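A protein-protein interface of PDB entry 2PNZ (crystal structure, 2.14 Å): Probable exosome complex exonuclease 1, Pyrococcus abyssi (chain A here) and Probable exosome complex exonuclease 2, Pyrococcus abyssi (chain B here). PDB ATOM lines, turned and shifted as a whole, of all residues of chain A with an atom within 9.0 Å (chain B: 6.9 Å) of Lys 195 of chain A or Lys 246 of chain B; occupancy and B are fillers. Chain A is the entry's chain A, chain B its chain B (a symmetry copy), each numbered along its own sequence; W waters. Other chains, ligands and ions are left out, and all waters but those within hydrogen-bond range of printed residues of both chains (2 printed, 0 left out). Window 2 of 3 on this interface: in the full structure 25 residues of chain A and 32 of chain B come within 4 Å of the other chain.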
ATOM      1  N   PRO A 111      18.866   5.983 -24.719  1.00  0.00           N
ATOM      2  CA  PRO A 111      18.924   7.348 -25.214  1.00  0.00           C
ATOM      3  C   PRO A 111      18.544   7.464 -26.709  1.00  0.00           C
ATOM      4  O   PRO A 111      18.321   8.543 -27.166  1.00  0.00           O
ATOM      5  CB  PRO A 111      20.384   7.770 -24.966  1.00  0.00           C
ATOM      6  CG  PRO A 111      21.107   6.561 -24.500  1.00  0.00           C
ATOM      7  CD  PRO A 111      20.173   5.470 -24.265  1.00  0.00           C
ATOM      8  N   ARG A 156      15.943   8.499 -32.154  1.00  0.00           N
ATOM      9  CA  ARG A 156      16.577   9.736 -32.525  1.00  0.00           C
ATOM     10  C   ARG A 156      17.711   9.415 -33.474  1.00  0.00           C
ATOM     11  O   ARG A 156      18.088  10.225 -34.323  1.00  0.00           O
ATOM     12  CB  ARG A 156      17.124  10.403 -31.284  1.00  0.00           C
ATOM     13  CG  ARG A 156      16.189  10.318 -30.138  1.00  0.00           C
ATOM     14  CD  ARG A 156      16.708  11.223 -29.071  1.00  0.00           C
ATOM     15  NE  ARG A 156      15.653  11.741 -28.219  1.00  0.00           N
ATOM     16  CZ  ARG A 156      15.138  11.080 -27.191  1.00  0.00           C
ATOM     17  NH1 ARG A 156      15.565   9.866 -26.887  1.00  0.00           N
ATOM     18  NH2 ARG A 156      14.203  11.654 -26.461  1.00  0.00           N
ATOM     19  N   ASP A 157      18.266   8.215 -33.288  1.00  0.00           N
ATOM     20  CA  ASP A 157      19.322   7.708 -34.117  1.00  0.00           C
ATOM     21  C   ASP A 157      19.259   6.233 -33.916  1.00  0.00           C
ATOM     22  O   ASP A 157      18.683   5.740 -32.913  1.00  0.00           O
ATOM     23  CB  ASP A 157      20.688   8.220 -33.642  1.00  0.00           C
ATOM     24  CG  ASP A 157      21.724   8.336 -34.787  1.00  0.00           C
ATOM     25  OD1 ASP A 157      21.546   7.762 -35.888  1.00  0.00           O
ATOM     26  OD2 ASP A 157      22.729   9.030 -34.560  1.00  0.00           O
ATOM     27  N   LEU A 158      19.838   5.512 -34.873  1.00  0.00           N
ATOM     28  CA  LEU A 158      20.307   4.151 -34.601  1.00  0.00           C
ATOM     29  C   LEU A 158      21.417   4.205 -33.583  1.00  0.00           C
ATOM     30  O   LEU A 158      22.093   5.220 -33.425  1.00  0.00           O
ATOM     31  CB  LEU A 158      20.819   3.482 -35.865  1.00  0.00           C
ATOM     32  CG  LEU A 158      19.739   3.268 -36.928  1.00  0.00           C
ATOM     33  CD1 LEU A 158      20.348   2.607 -38.156  1.00  0.00           C
ATOM     34  CD2 LEU A 158      18.592   2.456 -36.356  1.00  0.00           C
ATOM     35  N   ALA A 190      29.400   2.287 -27.931  1.00  0.00           N
ATOM     36  CA  ALA A 190      28.255   2.418 -28.806  1.00  0.00           C
ATOM     37  C   ALA A 190      27.955   3.851 -28.899  1.00  0.00           C
ATOM     38  O   ALA A 190      28.176   4.612 -27.965  1.00  0.00           O
ATOM     39  CB  ALA A 190      27.062   1.612 -28.307  1.00  0.00           C
ATOM     40  N   ILE A 191      27.505   4.248 -30.071  1.00  0.00           N
ATOM     41  CA  ILE A 191      27.205   5.642 -30.288  1.00  0.00           C
ATOM     42  C   ILE A 191      25.975   5.772 -31.063  1.00  0.00           C
ATOM     43  O   ILE A 191      25.595   4.877 -31.790  1.00  0.00           O
ATOM     44  CB  ILE A 191      28.314   6.405 -31.106  1.00  0.00           C
ATOM     45  CG1 ILE A 191      28.556   5.762 -32.463  1.00  0.00           C
ATOM     46  CG2 ILE A 191      29.542   6.544 -30.335  1.00  0.00           C
ATOM     47  CD1 ILE A 191      29.571   4.782 -32.408  1.00  0.00           C
ATOM     48  N   MET A 192      25.340   6.904 -30.924  1.00  0.00           N
ATOM     49  CA  MET A 192      24.367   7.340 -31.862  1.00  0.00           C
ATOM     50  C   MET A 192      25.197   8.224 -32.807  1.00  0.00           C
ATOM     51  O   MET A 192      25.561   9.361 -32.433  1.00  0.00           O
ATOM     52  CB  MET A 192      23.314   8.131 -31.108  1.00  0.00           C
ATOM     53  CG  MET A 192      22.507   7.274 -30.103  1.00  0.00           C
ATOM     54  SD  MET A 192      21.176   8.243 -29.416  1.00  0.00           S
ATOM     55  CE  MET A 192      22.009   9.204 -28.131  1.00  0.00           C
ATOM     56  N   PRO A 193      25.500   7.716 -34.021  1.00  0.00           N
ATOM     57  CA  PRO A 193      26.493   8.426 -34.900  1.00  0.00           C
ATOM     58  C   PRO A 193      26.108   9.832 -35.383  1.00  0.00           C
ATOM     59  O   PRO A 193      27.011  10.641 -35.674  1.00  0.00           O
ATOM     60  CB  PRO A 193      26.683   7.479 -36.089  1.00  0.00           C
ATOM     61  CG  PRO A 193      26.031   6.124 -35.633  1.00  0.00           C
ATOM     62  CD  PRO A 193      24.978   6.477 -34.639  1.00  0.00           C
ATOM     63  N   LEU A 194      24.813  10.153 -35.493  1.00  0.00           N
ATOM     64  CA  LEU A 194      24.456  11.459 -36.059  1.00  0.00           C
ATOM     65  C   LEU A 194      25.019  12.577 -35.227  1.00  0.00           C
ATOM     66  O   LEU A 194      25.590  13.545 -35.778  1.00  0.00           O
ATOM     67  CB  LEU A 194      22.958  11.618 -36.306  1.00  0.00           C
ATOM     68  CG  LEU A 194      22.488  10.803 -37.540  1.00  0.00           C
ATOM     69  CD1 LEU A 194      20.981  10.895 -37.780  1.00  0.00           C
ATOM     70  CD2 LEU A 194      23.261  11.169 -38.828  1.00  0.00           C
ATOM     71  N   LYS A 195      24.935  12.398 -33.908  1.00  0.00           N
ATOM     72  CA  LYS A 195      25.388  13.387 -32.970  1.00  0.00           C
ATOM     73  C   LYS A 195      26.648  12.967 -32.233  1.00  0.00           C
ATOM     74  O   LYS A 195      27.113  13.678 -31.332  1.00  0.00           O
ATOM     75  CB  LYS A 195      24.281  13.680 -31.971  1.00  0.00           C
ATOM     76  CG  LYS A 195      23.569  15.017 -32.171  1.00  0.00           C
ATOM     77  CD  LYS A 195      22.144  14.806 -32.670  1.00  0.00           C
ATOM     78  CE  LYS A 195      21.160  15.865 -32.123  1.00  0.00           C
ATOM     79  NZ  LYS A 195      20.750  15.571 -30.693  1.00  0.00           N
ATOM     80  N   ASN A 196      27.212  11.823 -32.608  1.00  0.00           N
ATOM     81  CA  ASN A 196      28.389  11.312 -31.928  1.00  0.00           C
ATOM     82  C   ASN A 196      28.140  11.151 -30.432  1.00  0.00           C
ATOM     83  O   ASN A 196      28.959  11.593 -29.613  1.00  0.00           O
ATOM     84  CB  ASN A 196      29.564  12.281 -32.097  1.00  0.00           C
ATOM     85  CG  ASN A 196      30.125  12.269 -33.500  1.00  0.00           C
ATOM     86  OD1 ASN A 196      30.972  11.422 -33.842  1.00  0.00           O
ATOM     87  ND2 ASN A 196      29.656  13.198 -34.325  1.00  0.00           N
ATOM     88  N   ASP A 197      27.006  10.574 -30.071  1.00  0.00           N
ATOM     89  CA  ASP A 197      26.627  10.539 -28.680  1.00  0.00           C
ATOM     90  C   ASP A 197      27.094   9.199 -28.208  1.00  0.00           C
ATOM     91  O   ASP A 197      26.752   8.227 -28.831  1.00  0.00           O
ATOM     92  CB  ASP A 197      25.118  10.717 -28.574  1.00  0.00           C
ATOM     93  CG  ASP A 197      24.709  12.206 -28.540  1.00  0.00           C
ATOM     94  OD1 ASP A 197      25.469  13.025 -27.993  1.00  0.00           O
ATOM     95  OD2 ASP A 197      23.622  12.552 -29.048  1.00  0.00           O
ATOM     96  N   ILE A 198      27.958   9.124 -27.190  1.00  0.00           N
ATOM     97  CA  ILE A 198      28.418   7.824 -26.785  1.00  0.00           C
ATOM     98  C   ILE A 198      27.451   7.262 -25.749  1.00  0.00           C
ATOM     99  O   ILE A 198      27.328   7.767 -24.620  1.00  0.00           O
ATOM    100  CB  ILE A 198      29.922   7.759 -26.338  1.00  0.00           C
ATOM    101  CG1 ILE A 198      30.883   8.149 -27.466  1.00  0.00           C
ATOM    102  CG2 ILE A 198      30.262   6.336 -25.812  1.00  0.00           C
ATOM    103  CD1 ILE A 198      32.167   8.860 -26.967  1.00  0.00           C
ATOM    104  N   THR A 199      26.787   6.162 -26.122  1.00  0.00           N
ATOM    105  CA  THR A 199      25.835   5.506 -25.200  1.00  0.00           C
ATOM    106  C   THR A 199      26.338   4.237 -24.514  1.00  0.00           C
ATOM    107  O   THR A 199      25.732   3.725 -23.564  1.00  0.00           O
ATOM    108  CB  THR A 199      24.470   5.274 -25.869  1.00  0.00           C
ATOM    109  OG1 THR A 199      24.570   4.234 -26.835  1.00  0.00           O
ATOM    110  CG2 THR A 199      23.959   6.558 -26.523  1.00  0.00           C
ATOM    111  N   LEU A 201      30.156   2.711 -23.090  1.00  0.00           N
ATOM    112  CA  LEU A 201      31.606   2.806 -23.120  1.00  0.00           C
ATOM    113  C   LEU A 201      32.083   1.991 -21.949  1.00  0.00           C
ATOM    114  O   LEU A 201      31.737   2.268 -20.840  1.00  0.00           O
ATOM    115  CB  LEU A 201      32.135   4.247 -23.046  1.00  0.00           C
ATOM    116  CG  LEU A 201      33.457   4.689 -23.727  1.00  0.00           C
ATOM    117  CD1 LEU A 201      34.180   5.799 -22.957  1.00  0.00           C
ATOM    118  CD2 LEU A 201      34.415   3.551 -23.905  1.00  0.00           C
ATOM    119  N   ILE A 213      41.816   6.598 -25.134  1.00  0.00           N
ATOM    120  CA  ILE A 213      41.215   7.537 -26.075  1.00  0.00           C
ATOM    121  C   ILE A 213      41.341   7.081 -27.547  1.00  0.00           C
ATOM    122  O   ILE A 213      40.357   7.146 -28.291  1.00  0.00           O
ATOM    123  CB  ILE A 213      41.738   8.995 -25.871  1.00  0.00           C
ATOM    124  CG1 ILE A 213      41.224   9.625 -24.554  1.00  0.00           C
ATOM    125  CG2 ILE A 213      41.447   9.892 -27.066  1.00  0.00           C
ATOM    126  CD1 ILE A 213      39.759   9.203 -24.127  1.00  0.00           C
ATOM    127  N   VAL A 216      38.819   4.275 -28.060  1.00  0.00           N
ATOM    128  CA  VAL A 216      37.526   4.925 -28.239  1.00  0.00           C
ATOM    129  C   VAL A 216      37.354   5.557 -29.631  1.00  0.00           C
ATOM    130  O   VAL A 216      36.402   5.195 -30.319  1.00  0.00           O
ATOM    131  CB  VAL A 216      37.220   5.884 -27.107  1.00  0.00           C
ATOM    132  CG1 VAL A 216      35.862   6.509 -27.270  1.00  0.00           C
ATOM    133  CG2 VAL A 216      37.292   5.126 -25.767  1.00  0.00           C
ATOM    134  N   ILE A 220      34.795   3.865 -32.497  1.00  0.00           N
ATOM    135  CA  ILE A 220      33.766   4.743 -33.028  1.00  0.00           C
ATOM    136  C   ILE A 220      33.805   4.712 -34.571  1.00  0.00           C
ATOM    137  O   ILE A 220      32.753   4.573 -35.202  1.00  0.00           O
ATOM    138  CB  ILE A 220      33.928   6.194 -32.497  1.00  0.00           C
ATOM    139  CG1 ILE A 220      33.577   6.254 -30.982  1.00  0.00           C
ATOM    140  CG2 ILE A 220      33.105   7.164 -33.328  1.00  0.00           C
ATOM    141  CD1 ILE A 220      33.976   7.564 -30.298  1.00  0.00           C
ATOM    142  N   LYS A 224      30.733   3.745 -36.841  1.00  0.00           N
ATOM    143  CA  LYS A 224      30.236   4.433 -38.019  1.00  0.00           C
ATOM    144  C   LYS A 224      30.217   3.550 -39.296  1.00  0.00           C
ATOM    145  O   LYS A 224      29.273   3.557 -40.047  1.00  0.00           O
ATOM    146  CB  LYS A 224      31.059   5.706 -38.249  1.00  0.00           C
ATOM    147  CG  LYS A 224      30.666   6.812 -37.248  1.00  0.00           C
ATOM    148  CD  LYS A 224      31.679   7.901 -37.164  1.00  0.00           C
ATOM    149  CE  LYS A 224      31.299   8.899 -36.084  1.00  0.00           C
ATOM    150  NZ  LYS A 224      32.173  10.089 -36.264  1.00  0.00           N
ATOM    151  N   TYR A 227      27.307   1.298 -38.656  1.00  0.00           N
ATOM    152  CA  TYR A 227      26.142   2.111 -38.860  1.00  0.00           C
ATOM    153  C   TYR A 227      25.752   2.185 -40.335  1.00  0.00           C
ATOM    154  O   TYR A 227      24.567   2.180 -40.652  1.00  0.00           O
ATOM    155  CB  TYR A 227      26.469   3.487 -38.380  1.00  0.00           C
ATOM    156  CG  TYR A 227      25.364   4.489 -38.489  1.00  0.00           C
ATOM    157  CD1 TYR A 227      24.215   4.362 -37.707  1.00  0.00           C
ATOM    158  CD2 TYR A 227      25.504   5.611 -39.317  1.00  0.00           C
ATOM    159  CE1 TYR A 227      23.211   5.332 -37.760  1.00  0.00           C
ATOM    160  CE2 TYR A 227      24.507   6.589 -39.393  1.00  0.00           C
ATOM    161  CZ  TYR A 227      23.363   6.446 -38.606  1.00  0.00           C
ATOM    162  OH  TYR A 227      22.358   7.402 -38.636  1.00  0.00           O
ATOM    163  N   LYS B 203      26.556  12.875 -15.521  1.00  0.00           N
ATOM    164  CA  LYS B 203      26.207  13.854 -16.491  1.00  0.00           C
ATOM    165  C   LYS B 203      24.779  14.345 -16.212  1.00  0.00           C
ATOM    166  O   LYS B 203      23.839  13.555 -16.127  1.00  0.00           O
ATOM    167  CB  LYS B 203      26.304  13.278 -17.908  1.00  0.00           C
ATOM    168  CG  LYS B 203      26.119  14.326 -18.986  1.00  0.00           C
ATOM    169  CD  LYS B 203      26.562  13.870 -20.361  1.00  0.00           C
ATOM    170  CE  LYS B 203      26.012  14.812 -21.417  1.00  0.00           C
ATOM    171  NZ  LYS B 203      26.610  14.415 -22.746  1.00  0.00           N
ATOM    172  N   ASN B 206      24.445  19.128 -19.835  1.00  0.00           N
ATOM    173  CA  ASN B 206      25.740  19.205 -20.486  1.00  0.00           C
ATOM    174  C   ASN B 206      26.895  19.364 -19.498  1.00  0.00           C
ATOM    175  O   ASN B 206      28.002  19.712 -19.882  1.00  0.00           O
ATOM    176  CB  ASN B 206      25.735  20.364 -21.484  1.00  0.00           C
ATOM    177  CG  ASN B 206      24.973  20.015 -22.746  1.00  0.00           C
ATOM    178  OD1 ASN B 206      25.025  18.866 -23.211  1.00  0.00           O
ATOM    179  ND2 ASN B 206      24.231  20.987 -23.290  1.00  0.00           N
ATOM    180  N   LEU B 208      29.223  17.553 -16.314  1.00  0.00           N
ATOM    181  CA  LEU B 208      29.609  16.402 -15.526  1.00  0.00           C
ATOM    182  C   LEU B 208      30.030  16.850 -14.164  1.00  0.00           C
ATOM    183  O   LEU B 208      30.743  17.813 -14.032  1.00  0.00           O
ATOM    184  CB  LEU B 208      30.793  15.595 -16.093  1.00  0.00           C
ATOM    185  CG  LEU B 208      30.909  15.155 -17.531  1.00  0.00           C
ATOM    186  CD1 LEU B 208      31.645  13.872 -17.538  1.00  0.00           C
ATOM    187  CD2 LEU B 208      29.586  15.089 -18.310  1.00  0.00           C
ATOM    188  N   ALA B 244      24.242   9.836 -22.768  1.00  0.00           N
ATOM    189  CA  ALA B 244      25.256   9.717 -23.803  1.00  0.00           C
ATOM    190  C   ALA B 244      26.323  10.677 -23.373  1.00  0.00           C
ATOM    191  O   ALA B 244      26.018  11.666 -22.731  1.00  0.00           O
ATOM    192  CB  ALA B 244      24.700  10.088 -25.147  1.00  0.00           C
ATOM    193  N   PHE B 245      27.571  10.343 -23.631  1.00  0.00           N
ATOM    194  CA  PHE B 245      28.679  11.247 -23.398  1.00  0.00           C
ATOM    195  C   PHE B 245      29.282  11.617 -24.726  1.00  0.00           C
ATOM    196  O   PHE B 245      29.188  10.855 -25.700  1.00  0.00           O
ATOM    197  CB  PHE B 245      29.713  10.621 -22.464  1.00  0.00           C
ATOM    198  CG  PHE B 245      29.217  10.474 -21.028  1.00  0.00           C
ATOM    199  CD1 PHE B 245      29.574  11.397 -20.063  1.00  0.00           C
ATOM    200  CD2 PHE B 245      28.327   9.464 -20.685  1.00  0.00           C
ATOM    201  CE1 PHE B 245      29.110  11.281 -18.776  1.00  0.00           C
ATOM    202  CE2 PHE B 245      27.870   9.317 -19.404  1.00  0.00           C
ATOM    203  CZ  PHE B 245      28.300  10.221 -18.420  1.00  0.00           C
ATOM    204  N   LYS B 246      29.877  12.802 -24.766  1.00  0.00           N
ATOM    205  CA  LYS B 246      30.636  13.252 -25.912  1.00  0.00           C
ATOM    206  C   LYS B 246      32.037  12.685 -25.700  1.00  0.00           C
ATOM    207  O   LYS B 246      32.397  12.437 -24.565  1.00  0.00           O
ATOM    208  CB  LYS B 246      30.651  14.769 -25.907  1.00  0.00           C
ATOM    209  CG  LYS B 246      29.682  15.462 -26.900  1.00  0.00           C
ATOM    210  CD  LYS B 246      28.363  14.763 -27.009  1.00  0.00           C
ATOM    211  CE  LYS B 246      27.391  15.484 -27.961  1.00  0.00           C
ATOM    212  NZ  LYS B 246      27.796  15.253 -29.356  1.00  0.00           N
ATOM    213  N   LEU B 247      32.792  12.462 -26.776  1.00  0.00           N
ATOM    214  CA  LEU B 247      34.206  12.068 -26.659  1.00  0.00           C
ATOM    215  C   LEU B 247      34.974  12.991 -25.716  1.00  0.00           C
ATOM    216  O   LEU B 247      35.687  12.507 -24.832  1.00  0.00           O
ATOM    217  CB  LEU B 247      34.950  12.082 -27.990  1.00  0.00           C
ATOM    218  CG  LEU B 247      36.111  11.086 -28.202  1.00  0.00           C
ATOM    219  CD1 LEU B 247      36.958  11.454 -29.349  1.00  0.00           C
ATOM    220  CD2 LEU B 247      37.024  10.802 -27.051  1.00  0.00           C
ATOM    221  N   GLU B 248      34.863  14.306 -25.929  1.00  0.00           N
ATOM    222  CA  GLU B 248      35.513  15.274 -25.057  1.00  0.00           C
ATOM    223  C   GLU B 248      35.014  15.177 -23.628  1.00  0.00           C
ATOM    224  O   GLU B 248      35.762  15.382 -22.726  1.00  0.00           O
ATOM    225  CB  GLU B 248      35.490  16.717 -25.607  1.00  0.00           C
ATOM    226  CG  GLU B 248      34.308  17.112 -26.439  1.00  0.00           C
ATOM    227  CD  GLU B 248      34.174  16.316 -27.740  1.00  0.00           C
ATOM    228  OE1 GLU B 248      35.144  16.299 -28.564  1.00  0.00           O
ATOM    229  OE2 GLU B 248      33.073  15.724 -27.933  1.00  0.00           O
ATOM    230  N   GLU B 249      33.780  14.790 -23.400  1.00  0.00           N
ATOM    231  CA  GLU B 249      33.330  14.523 -21.999  1.00  0.00           C
ATOM    232  C   GLU B 249      34.096  13.423 -21.358  1.00  0.00           C
ATOM    233  O   GLU B 249      34.520  13.518 -20.201  1.00  0.00           O
ATOM    234  CB  GLU B 249      31.865  14.226 -21.958  1.00  0.00           C
ATOM    235  CG  GLU B 249      31.100  15.521 -22.099  1.00  0.00           C
ATOM    236  CD  GLU B 249      29.634  15.353 -22.273  1.00  0.00           C
ATOM    237  OE1 GLU B 249      29.135  14.223 -22.551  1.00  0.00           O
ATOM    238  OE2 GLU B 249      28.972  16.401 -22.155  1.00  0.00           O
ATOM    239  N   VAL B 250      34.305  12.391 -22.155  1.00  0.00           N
ATOM    240  CA  VAL B 250      35.009  11.194 -21.740  1.00  0.00           C
ATOM    241  C   VAL B 250      36.502  11.532 -21.440  1.00  0.00           C
ATOM    242  O   VAL B 250      37.026  11.195 -20.376  1.00  0.00           O
ATOM    243  CB  VAL B 250      34.794  10.058 -22.789  1.00  0.00           C
ATOM    244  CG1 VAL B 250      35.918   8.976 -22.683  1.00  0.00           C
ATOM    245  CG2 VAL B 250      33.360   9.465 -22.615  1.00  0.00           C
ATOM    246  N   MET B 251      37.136  12.239 -22.362  1.00  0.00           N
ATOM    247  CA  MET B 251      38.512  12.722 -22.207  1.00  0.00           C
ATOM    248  C   MET B 251      38.751  13.470 -20.897  1.00  0.00           C
ATOM    249  O   MET B 251      39.658  13.147 -20.162  1.00  0.00           O
ATOM    250  CB  MET B 251      38.868  13.611 -23.389  1.00  0.00           C
ATOM    251  CG  MET B 251      38.740  12.914 -24.739  1.00  0.00           C
ATOM    252  SD  MET B 251      38.957  13.904 -26.269  1.00  0.00           S
ATOM    253  CE  MET B 251      40.345  14.976 -25.916  1.00  0.00           C
HETATM  254  O   HOH W   1      31.639  12.082 -29.382  1.00  0.00           O
HETATM  255  O   HOH W   2      26.065  13.605 -25.658  1.00  0.00           O
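Among the printed residues, merely in contact across the chains: Ile 198 of chain A with Ala 244 of chain B, Asp 197 of chain A with Ala 244 of chain B, Leu 201 of chain A with Val 250 of chain B, Ile 198 of chain A with Leu 247 of chain B, Asp 197 of chain A with Phe 245 of chain B, Asn 196 of chain A with Lys 246 of chain B, Thr 199 of chain A with Ala 244 of chain B, Ile 213 of chain A with Met 251 of chain B and Asn 196 of chain A with Phe 245 of chain B.
Of the 20 printed residues of chain A, 7 touch a printed residue of chain B. Hydrophobic or aromatic side chains of chain A that line the printed part of chain B: Ile 198, Leu 201 and Ile 213. Printed residues of chain B that touch a printed residue of chain A: Ala 244, Phe 245, Lys 246, Leu 247, Val 250 and Met 251. Hydrophobic or aromatic side chains of chain B within 4 Å of the printed part of chain A: Ala 244, Val 250 and Met 251. Among the printed residues, 12 pairs touch across the chains. Among the printed residues, Asp or Glu carboxylates within 4 Å of a Lys or Arg side-chain nitrogen of the other chain: Asp 197 of chain A with Lys 246 of chain B (3.5 Å).
Lys 195 of chain A touches one residue of chain B. Of chain A, only Lys 195 (2.6 Å), Asn 196 (3.8 Å) and Asp 197 (3.1 Å) come within 4 Å of Lys 246 of chain B. Printed residues of chain A within 4 Å of Phe 245 of chain B: Asn 196, Asp 197 and Ile 198. Printed residues of chain B within 4 Å of Ile 213 of chain A: Met 251. Of the printed residues of chain B, Ile 198 of chain A touches Ala 244 (3.0 Å), Phe 245 (2.6 Å) and Leu 247 (3.7 Å). Printed residues of chain A within 4 Å of Met 251 of chain B: Ile 213 (3.9 Å). Of the printed residues of chain B, Asp 197 of chain A touches Ala 244 (3.5 Å), Phe 245 (3.7 Å) and Lys 246 (3.1 Å). Ala 190 of chain A touches none of the printed residues of chain B. Leu 194 of chain A touches none of the printed residues of chain B. The nearest residue of chain A that does not touch Lys 246 of chain B is Ile 198 of chain A (4.03 Å). The nearest printed residue of chain A that does not touch Leu 247 of chain B is Ile 213 of chain A (4.3 Å).
The side-chain carboxylate (OE1) of Glu 249 of chain B is in hydrogen-bond range of the backbone NH (N) of Lys 246 of chain B, at 2.7 Å. The backbone NH of Met 192 of chain A sits at hydrogen-bond distance from the backbone carbonyl oxygen of Asp 197 of chain A (2.9 Å). The backbone carbonyl oxygen of Ala 190 of chain A lies within hydrogen-bond range of the backbone NH of Thr 199 of chain A (2.8 Å). The side-chain amide oxygen (OD1) of Asn 196 of chain A sits at hydrogen-bond distance from the side-chain amino group (NZ) of Lys 224 of chain A (3.0 Å). The backbone carbonyl oxygen (O) of Ala 244 of chain B lies within hydrogen-bond range of the side-chain amino group (NZ) of Lys 203 of chain B (2.8 Å).
NZ of Lys 246 of chain B is in salt-bridge range of OD1 of Asp 197 of chain A, 3.5 Å away. N of Ile 198 of chain A lies within hydrogen-bond range of O of Phe 245 of chain B, at 2.6 Å. The backbone carbonyl oxygen of Lys 195 of chain A lies within hydrogen-bond range of the side-chain amino group of Lys 246 of chain B, 2.6 Å away.
Water W2 bridges OD1 of Asp 197 of chain A and NZ of Lys 203 of chain B. Water W1 lies within hydrogen-bond range of the backbone carbonyl oxygen of Asn 196 of chain A and the backbone NH of Leu 247 of chain B.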
